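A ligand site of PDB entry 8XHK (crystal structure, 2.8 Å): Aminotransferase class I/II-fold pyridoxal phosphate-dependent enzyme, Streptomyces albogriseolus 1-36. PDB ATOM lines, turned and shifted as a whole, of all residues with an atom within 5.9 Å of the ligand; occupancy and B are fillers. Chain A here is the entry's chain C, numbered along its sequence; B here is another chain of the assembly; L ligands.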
ATOM      1  N   TYR A  47      -3.058   3.007 -18.528  1.00  0.00           N
ATOM      2  CA  TYR A  47      -2.943   3.080 -17.078  1.00  0.00           C
ATOM      3  C   TYR A  47      -4.293   3.180 -16.378  1.00  0.00           C
ATOM      4  O   TYR A  47      -4.358   2.971 -15.162  1.00  0.00           O
ATOM      5  CB  TYR A  47      -2.093   4.289 -16.680  1.00  0.00           C
ATOM      6  CG  TYR A  47      -0.597   4.072 -16.759  1.00  0.00           C
ATOM      7  CD1 TYR A  47       0.115   3.580 -15.675  1.00  0.00           C
ATOM      8  CD2 TYR A  47       0.111   4.372 -17.919  1.00  0.00           C
ATOM      9  CE1 TYR A  47       1.486   3.385 -15.738  1.00  0.00           C
ATOM     10  CE2 TYR A  47       1.476   4.191 -17.990  1.00  0.00           C
ATOM     11  CZ  TYR A  47       2.165   3.704 -16.902  1.00  0.00           C
ATOM     12  OH  TYR A  47       3.517   3.510 -16.973  1.00  0.00           O
ATOM     13  N   ASN A 105      -1.019  19.362  -9.121  1.00  0.00           N
ATOM     14  CA  ASN A 105      -1.105  19.113 -10.563  1.00  0.00           C
ATOM     15  C   ASN A 105      -0.524  17.773 -10.977  1.00  0.00           C
ATOM     16  O   ASN A 105      -0.758  17.347 -12.115  1.00  0.00           O
ATOM     17  CB  ASN A 105      -0.411  20.241 -11.336  1.00  0.00           C
ATOM     18  CG  ASN A 105       0.948  20.581 -10.774  1.00  0.00           C
ATOM     19  OD1 ASN A 105       1.929  19.876 -11.015  1.00  0.00           O
ATOM     20  ND2 ASN A 105       1.020  21.672 -10.012  1.00  0.00           N
ATOM     21  N   SER A 106       0.206  17.085 -10.093  1.00  0.00           N
ATOM     22  CA  SER A 106       0.792  15.790 -10.434  1.00  0.00           C
ATOM     23  C   SER A 106       1.305  15.141  -9.156  1.00  0.00           C
ATOM     24  O   SER A 106       1.599  15.821  -8.176  1.00  0.00           O
ATOM     25  CB  SER A 106       1.928  15.933 -11.444  1.00  0.00           C
ATOM     26  OG  SER A 106       3.023  16.644 -10.898  1.00  0.00           O
ATOM     27  N   CYS A 107       1.408  13.808  -9.202  1.00  0.00           N
ATOM     28  CA  CYS A 107       2.004  13.085  -8.081  1.00  0.00           C
ATOM     29  C   CYS A 107       3.466  13.461  -7.890  1.00  0.00           C
ATOM     30  O   CYS A 107       3.969  13.439  -6.759  1.00  0.00           O
ATOM     31  CB  CYS A 107       1.860  11.573  -8.292  1.00  0.00           C
ATOM     32  SG  CYS A 107       2.522  10.553  -6.954  1.00  0.00           S
ATOM     33  N   SER A 108       4.156  13.802  -8.976  1.00  0.00           N
ATOM     34  CA  SER A 108       5.543  14.253  -8.852  1.00  0.00           C
ATOM     35  C   SER A 108       5.629  15.545  -8.043  1.00  0.00           C
ATOM     36  O   SER A 108       6.520  15.698  -7.193  1.00  0.00           O
ATOM     37  CB  SER A 108       6.145  14.454 -10.242  1.00  0.00           C
ATOM     38  OG  SER A 108       6.040  13.275 -11.015  1.00  0.00           O
ATOM     39  N   ALA A 109       4.698  16.480  -8.278  1.00  0.00           N
ATOM     40  CA  ALA A 109       4.671  17.703  -7.494  1.00  0.00           C
ATOM     41  C   ALA A 109       4.389  17.420  -6.026  1.00  0.00           C
ATOM     42  O   ALA A 109       4.800  18.209  -5.157  1.00  0.00           O
ATOM     43  CB  ALA A 109       3.627  18.670  -8.053  1.00  0.00           C
ATOM     44  N   HIS A 138      10.069   4.972  -6.928  1.00  0.00           N
ATOM     45  CA  HIS A 138       9.879   5.636  -8.198  1.00  0.00           C
ATOM     46  C   HIS A 138      10.835   6.816  -8.346  1.00  0.00           C
ATOM     47  O   HIS A 138      11.330   7.380  -7.370  1.00  0.00           O
ATOM     48  CB  HIS A 138       8.436   6.102  -8.368  1.00  0.00           C
ATOM     49  CG  HIS A 138       8.069   6.454  -9.778  1.00  0.00           C
ATOM     50  ND1 HIS A 138       8.093   7.748 -10.249  1.00  0.00           N
ATOM     51  CD2 HIS A 138       7.697   5.679 -10.816  1.00  0.00           C
ATOM     52  CE1 HIS A 138       7.737   7.754 -11.526  1.00  0.00           C
ATOM     53  NE2 HIS A 138       7.489   6.508 -11.891  1.00  0.00           N
ATOM     54  N   CYS A 140      10.375   9.865  -9.380  1.00  0.00           N
ATOM     55  CA  CYS A 140       9.934  11.179  -8.917  1.00  0.00           C
ATOM     56  C   CYS A 140      10.309  11.427  -7.466  1.00  0.00           C
ATOM     57  O   CYS A 140      10.360  12.575  -7.035  1.00  0.00           O
ATOM     58  CB  CYS A 140       8.424  11.344  -9.099  1.00  0.00           C
ATOM     59  SG  CYS A 140       7.402  10.456  -7.894  1.00  0.00           S
ATOM     60  N   ASP A 180       7.284   2.515  -2.611  1.00  0.00           N
ATOM     61  CA  ASP A 180       6.026   2.360  -3.337  1.00  0.00           C
ATOM     62  C   ASP A 180       5.157   1.345  -2.620  1.00  0.00           C
ATOM     63  O   ASP A 180       5.656   0.364  -2.059  1.00  0.00           O
ATOM     64  CB  ASP A 180       6.266   1.911  -4.781  1.00  0.00           C
ATOM     65  CG  ASP A 180       7.082   2.901  -5.582  1.00  0.00           C
ATOM     66  OD1 ASP A 180       7.636   3.848  -4.978  1.00  0.00           O
ATOM     67  OD2 ASP A 180       7.177   2.727  -6.820  1.00  0.00           O
ATOM     68  N   VAL A 182       2.868  -0.314  -4.419  1.00  0.00           N
ATOM     69  CA  VAL A 182       2.838  -1.311  -5.477  1.00  0.00           C
ATOM     70  C   VAL A 182       3.940  -0.986  -6.460  1.00  0.00           C
ATOM     71  O   VAL A 182       4.067   0.158  -6.913  1.00  0.00           O
ATOM     72  CB  VAL A 182       1.471  -1.366  -6.188  1.00  0.00           C
ATOM     73  CG1 VAL A 182       1.526  -2.289  -7.388  1.00  0.00           C
ATOM     74  CG2 VAL A 182       0.386  -1.817  -5.213  1.00  0.00           C
ATOM     75  N   SER A 184       5.550  -1.483 -10.101  1.00  0.00           N
ATOM     76  CA  SER A 184       5.136  -1.859 -11.451  1.00  0.00           C
ATOM     77  C   SER A 184       6.033  -2.960 -12.014  1.00  0.00           C
ATOM     78  O   SER A 184       5.582  -4.085 -12.264  1.00  0.00           O
ATOM     79  CB  SER A 184       5.143  -0.626 -12.359  1.00  0.00           C
ATOM     80  OG  SER A 184       6.413  -0.007 -12.347  1.00  0.00           O
ATOM     81  N   ASP A 209       4.167   5.674  -2.103  1.00  0.00           N
ATOM     82  CA  ASP A 209       3.673   6.115  -3.404  1.00  0.00           C
ATOM     83  C   ASP A 209       2.588   5.131  -3.830  1.00  0.00           C
ATOM     84  O   ASP A 209       2.881   3.967  -4.152  1.00  0.00           O
ATOM     85  CB  ASP A 209       4.807   6.173  -4.422  1.00  0.00           C
ATOM     86  CG  ASP A 209       4.399   6.874  -5.711  1.00  0.00           C
ATOM     87  OD1 ASP A 209       3.226   6.792  -6.109  1.00  0.00           O
ATOM     88  OD2 ASP A 209       5.274   7.507  -6.339  1.00  0.00           O
ATOM     89  N   ALA A 211       0.528   5.203  -6.476  1.00  0.00           N
ATOM     90  CA  ALA A 211       0.067   5.493  -7.826  1.00  0.00           C
ATOM     91  C   ALA A 211      -0.571   4.269  -8.474  1.00  0.00           C
ATOM     92  O   ALA A 211      -1.629   4.379  -9.121  1.00  0.00           O
ATOM     93  CB  ALA A 211       1.214   6.009  -8.680  1.00  0.00           C
ATOM     94  N   HIS A 212       0.050   3.106  -8.335  1.00  0.00           N
ATOM     95  CA  HIS A 212      -0.496   1.863  -8.868  1.00  0.00           C
ATOM     96  C   HIS A 212      -1.373   1.125  -7.859  1.00  0.00           C
ATOM     97  O   HIS A 212      -1.715  -0.038  -8.091  1.00  0.00           O
ATOM     98  CB  HIS A 212       0.626   0.941  -9.348  1.00  0.00           C
ATOM     99  CG  HIS A 212       1.337   1.441 -10.562  1.00  0.00           C
ATOM    100  ND1 HIS A 212       0.704   1.596 -11.780  1.00  0.00           N
ATOM    101  CD2 HIS A 212       2.621   1.820 -10.750  1.00  0.00           C
ATOM    102  CE1 HIS A 212       1.575   2.044 -12.660  1.00  0.00           C
ATOM    103  NE2 HIS A 212       2.736   2.191 -12.067  1.00  0.00           N
ATOM    104  N   THR A 240       0.006  10.072  -4.271  1.00  0.00           N
ATOM    105  CA  THR A 240      -0.602   9.241  -5.299  1.00  0.00           C
ATOM    106  C   THR A 240      -0.896  10.074  -6.530  1.00  0.00           C
ATOM    107  O   THR A 240      -0.904  11.311  -6.490  1.00  0.00           O
ATOM    108  CB  THR A 240      -1.887   8.574  -4.787  1.00  0.00           C
ATOM    109  OG1 THR A 240      -2.243   7.491  -5.648  1.00  0.00           O
ATOM    110  CG2 THR A 240      -3.037   9.579  -4.747  1.00  0.00           C
ATOM    111  N   SER A 241      -1.137   9.380  -7.638  1.00  0.00           N
ATOM    112  CA  SER A 241      -1.553   9.987  -8.893  1.00  0.00           C
ATOM    113  C   SER A 241      -3.030   9.711  -9.114  1.00  0.00           C
ATOM    114  O   SER A 241      -3.495   8.581  -8.914  1.00  0.00           O
ATOM    115  CB  SER A 241      -0.740   9.432 -10.062  1.00  0.00           C
ATOM    116  OG  SER A 241      -1.319   9.781 -11.304  1.00  0.00           O
ATOM    117  N   LEU A 242      -3.770  10.731  -9.535  1.00  0.00           N
ATOM    118  CA  LEU A 242      -5.212  10.646  -9.680  1.00  0.00           C
ATOM    119  C   LEU A 242      -5.663  10.460 -11.121  1.00  0.00           C
ATOM    120  O   LEU A 242      -6.836  10.680 -11.427  1.00  0.00           O
ATOM    121  CB  LEU A 242      -5.870  11.889  -9.072  1.00  0.00           C
ATOM    122  CG  LEU A 242      -5.733  12.046  -7.557  1.00  0.00           C
ATOM    123  CD1 LEU A 242      -6.424  13.309  -7.099  1.00  0.00           C
ATOM    124  CD2 LEU A 242      -6.300  10.838  -6.839  1.00  0.00           C
ATOM    125  N   ASN A 243      -4.758  10.073 -12.020  1.00  0.00           N
ATOM    126  CA  ASN A 243      -5.136   9.829 -13.409  1.00  0.00           C
ATOM    127  C   ASN A 243      -4.779   8.426 -13.895  1.00  0.00           C
ATOM    128  O   ASN A 243      -4.789   8.170 -15.102  1.00  0.00           O
ATOM    129  CB  ASN A 243      -4.494  10.874 -14.332  1.00  0.00           C
ATOM    130  CG  ASN A 243      -3.028  10.608 -14.605  1.00  0.00           C
ATOM    131  OD1 ASN A 243      -2.304  10.081 -13.763  1.00  0.00           O
ATOM    132  ND2 ASN A 243      -2.581  10.959 -15.808  1.00  0.00           N
ATOM    133  N   LYS A 244      -4.466   7.496 -12.982  1.00  0.00           N
ATOM    134  CA  LYS A 244      -4.135   6.114 -13.323  1.00  0.00           C
ATOM    135  C   LYS A 244      -5.068   5.217 -12.517  1.00  0.00           C
ATOM    136  O   LYS A 244      -4.695   4.692 -11.457  1.00  0.00           O
ATOM    137  CB  LYS A 244      -2.658   5.786 -13.033  1.00  0.00           C
ATOM    138  CG  LYS A 244      -1.702   6.934 -13.209  1.00  0.00           C
ATOM    139  CD  LYS A 244      -0.403   6.697 -12.457  1.00  0.00           C
ATOM    140  CE  LYS A 244       0.633   6.001 -13.321  1.00  0.00           C
ATOM    141  NZ  LYS A 244       1.901   5.762 -12.572  1.00  0.00           N
ATOM    142  N   GLY A 250      -4.075  15.021 -12.118  1.00  0.00           N
ATOM    143  CA  GLY A 250      -3.256  15.485 -11.024  1.00  0.00           C
ATOM    144  C   GLY A 250      -2.929  14.402 -10.012  1.00  0.00           C
ATOM    145  O   GLY A 250      -3.143  13.208 -10.214  1.00  0.00           O
ATOM    146  N   GLY A 251      -2.370  14.856  -8.894  1.00  0.00           N
ATOM    147  CA  GLY A 251      -2.024  13.979  -7.795  1.00  0.00           C
ATOM    148  C   GLY A 251      -2.527  14.511  -6.462  1.00  0.00           C
ATOM    149  O   GLY A 251      -3.276  15.490  -6.425  1.00  0.00           O
ATOM    150  N   ARG B  78      -2.255   7.369 -20.688  1.00  0.00           N
ATOM    151  CA  ARG B  78      -0.943   7.628 -20.103  1.00  0.00           C
ATOM    152  C   ARG B  78       0.153   6.742 -20.697  1.00  0.00           C
ATOM    153  O   ARG B  78       1.208   6.555 -20.078  1.00  0.00           O
ATOM    154  CB  ARG B  78      -0.979   7.504 -18.578  1.00  0.00           C
ATOM    155  CG  ARG B  78       0.093   8.281 -17.864  1.00  0.00           C
ATOM    156  CD  ARG B  78       0.282   7.748 -16.469  1.00  0.00           C
ATOM    157  NE  ARG B  78      -0.170   8.695 -15.459  1.00  0.00           N
ATOM    158  CZ  ARG B  78       0.605   9.601 -14.898  1.00  0.00           C
ATOM    159  NH1 ARG B  78       1.876   9.741 -15.246  1.00  0.00           N
ATOM    160  NH2 ARG B  78       0.105  10.394 -13.951  1.00  0.00           N
ATOM    161  N   ASN B 105       2.704  20.016 -17.011  1.00  0.00           N
ATOM    162  CA  ASN B 105       1.607  20.385 -16.123  1.00  0.00           C
ATOM    163  C   ASN B 105       1.855  21.675 -15.363  1.00  0.00           C
ATOM    164  O   ASN B 105       0.903  22.229 -14.799  1.00  0.00           O
ATOM    165  CB  ASN B 105       1.328  19.232 -15.152  1.00  0.00           C
ATOM    166  CG  ASN B 105       2.594  18.660 -14.548  1.00  0.00           C
ATOM    167  OD1 ASN B 105       3.223  19.278 -13.679  1.00  0.00           O
ATOM    168  ND2 ASN B 105       2.981  17.476 -14.995  1.00  0.00           N
ATOM    169  N   TRP B 276       7.875  10.757 -17.199  1.00  0.00           N
ATOM    170  CA  TRP B 276       6.951   9.993 -16.369  1.00  0.00           C
ATOM    171  C   TRP B 276       5.782  10.812 -15.818  1.00  0.00           C
ATOM    172  O   TRP B 276       4.722  10.236 -15.545  1.00  0.00           O
ATOM    173  CB  TRP B 276       7.692   9.343 -15.196  1.00  0.00           C
ATOM    174  CG  TRP B 276       8.501  10.312 -14.370  1.00  0.00           C
ATOM    175  CD1 TRP B 276       8.029  11.166 -13.404  1.00  0.00           C
ATOM    176  CD2 TRP B 276       9.914  10.504 -14.425  1.00  0.00           C
ATOM    177  NE1 TRP B 276       9.064  11.885 -12.869  1.00  0.00           N
ATOM    178  CE2 TRP B 276      10.236  11.496 -13.468  1.00  0.00           C
ATOM    179  CE3 TRP B 276      10.944   9.935 -15.179  1.00  0.00           C
ATOM    180  CZ2 TRP B 276      11.544  11.935 -13.265  1.00  0.00           C
ATOM    181  CZ3 TRP B 276      12.238  10.380 -14.967  1.00  0.00           C
ATOM    182  CH2 TRP B 276      12.529  11.369 -14.013  1.00  0.00           C
ATOM    183  N   SER B 277       5.935  12.116 -15.635  1.00  0.00           N
ATOM    184  CA  SER B 277       4.847  12.907 -15.073  1.00  0.00           C
ATOM    185  C   SER B 277       3.747  13.116 -16.099  1.00  0.00           C
ATOM    186  O   SER B 277       4.014  13.263 -17.292  1.00  0.00           O
ATOM    187  CB  SER B 277       5.355  14.255 -14.565  1.00  0.00           C
ATOM    188  OG  SER B 277       4.351  14.957 -13.853  1.00  0.00           O
ATOM    189  N   GLN B 278       2.499  13.113 -15.634  1.00  0.00           N
ATOM    190  CA  GLN B 278       1.357  13.200 -16.523  1.00  0.00           C
ATOM    191  C   GLN B 278       1.376  14.496 -17.321  1.00  0.00           C
ATOM    192  O   GLN B 278       1.887  15.525 -16.864  1.00  0.00           O
ATOM    193  CB  GLN B 278       0.052  13.088 -15.729  1.00  0.00           C
ATOM    194  CG  GLN B 278      -0.103  14.125 -14.638  1.00  0.00           C
ATOM    195  CD  GLN B 278      -1.370  13.938 -13.839  1.00  0.00           C
ATOM    196  OE1 GLN B 278      -2.450  14.353 -14.259  1.00  0.00           O
ATOM    197  NE2 GLN B 278      -1.246  13.309 -12.666  1.00  0.00           N
HETATM  198  N1  LIG L   1       4.564   7.381  -9.023  1.00  0.00           N
HETATM  199  C1  LIG L   1       4.541   6.066  -9.442  1.00  0.00           C
HETATM  200  C2  LIG L   1       5.056   4.979  -8.541  1.00  0.00           C
HETATM  201  C3  LIG L   1       4.033   5.742 -10.688  1.00  0.00           C
HETATM  202  O1  LIG L   1       4.009   4.436 -11.103  1.00  0.00           O
HETATM  203  C4  LIG L   1       3.551   6.737 -11.524  1.00  0.00           C
HETATM  204  C5  LIG L   1       3.130   6.407 -12.928  1.00  0.00           C
HETATM  205  C6  LIG L   1       3.586   8.065 -11.105  1.00  0.00           C
HETATM  206  C7  LIG L   1       4.090   8.385  -9.851  1.00  0.00           C
HETATM  207  C8  LIG L   1       3.061   9.162 -12.006  1.00  0.00           C
HETATM  208  O2  LIG L   1       3.171  10.420 -11.360  1.00  0.00           O
HETATM  209  P1  LIG L   1       2.518  11.737 -12.026  1.00  0.00           P
HETATM  210  O3  LIG L   1       2.414  11.542 -13.521  1.00  0.00           O
HETATM  211  O4  LIG L   1       3.370  12.940 -11.739  1.00  0.00           O
HETATM  212  O5  LIG L   1       1.132  11.937 -11.461  1.00  0.00           O
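NZ of Lys 244 is covalently linked to C5 of the ligand (1.4 Å).
The guanidinium group of Arg 78 of chain B lies within salt-bridge range of an oxygen (O3) of the ligand (2.6 Å).
N of Gln 278 of chain B lies within hydrogen-bond range of O3 of the ligand (2.6 Å).
The side-chain amide nitrogen of Gln 278 of chain B lies within hydrogen-bond range of an oxygen (O5) of the ligand (3.0 Å).
A ring nitrogen (NE2) of His 212 sits at hydrogen-bond distance from an oxygen (O1) of the ligand (2.8 Å).
A nitrogen (N1) of the ligand sits at hydrogen-bond distance from the side-chain carboxylate of Asp 209.
N of Ser 108 lies within hydrogen-bond range of O4 of the ligand (3.0 Å).
OG of Ser 108 sits at hydrogen-bond distance from O4 of the ligand (2.8 Å).
N of Cys 107 sits at hydrogen-bond distance from O5 of the ligand (2.9 Å).
An oxygen (O4) of the ligand sits at hydrogen-bond distance from the side-chain hydroxyl of Ser 277 of chain B (3.1 Å).
The side-chain hydroxyl (OG) of Ser 241 sits at hydrogen-bond distance from an oxygen (O5) of the ligand (3.3 Å).
The guanidinium group of Arg 78 of chain B sits close to the side-chain amide nitrogen of Gln 278 of chain B (3.5 Å).
The guanidinium group (NH2) of Arg 78 of chain B lies within hydrogen-bond range of the side-chain hydroxyl (OG) of Ser 241 (3.1 Å).
OD1 of Asn 243 sits at hydrogen-bond distance from NH2 of Arg 78 of chain B, at 2.4 Å.
The side-chain amide oxygen of Gln 278 of chain B lies within hydrogen-bond range of the backbone NH of Gly 250 (2.8 Å).
The side-chain carboxylate of Asp 209 is in hydrogen-bond range of the backbone NH of Ala 211 (3.2 Å).
The side-chain hydroxyl of Ser 277 of chain B lies within hydrogen-bond range of the side-chain amide nitrogen of Asn 105 of chain B (3.1 Å).
The side-chain hydroxyl (OG) of Ser 241 is in hydrogen-bond range of the side-chain amide oxygen (OD1) of Asn 243.
N of Ala 109 is in hydrogen-bond range of OG of Ser 106 (3.1 Å).
An oxygen (O3) of the ligand lies close to the backbone carbonyl oxygen of Trp 276 of chain B, 3.3 Å away.
Residues that only touch the ligand: Ser 106, His 138, Asp 180 and Ala 211.
Hydrophobic or aromatic side chains that line the ligand: His 138, Ala 211 and His 212.
14 residues have an atom within 4 Å of the ligand: Ser 106, Cys 107, Ser 108, His 138, Asp 180, Asp 209, Ala 211, His 212, Ser 241, Lys 244, Arg 78 of chain B, Trp 276 of chain B, Ser 277 of chain B and Gln 278 of chain B.
The nearest printed residue that does not touch the ligand is Cys 140 (4.3 Å).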
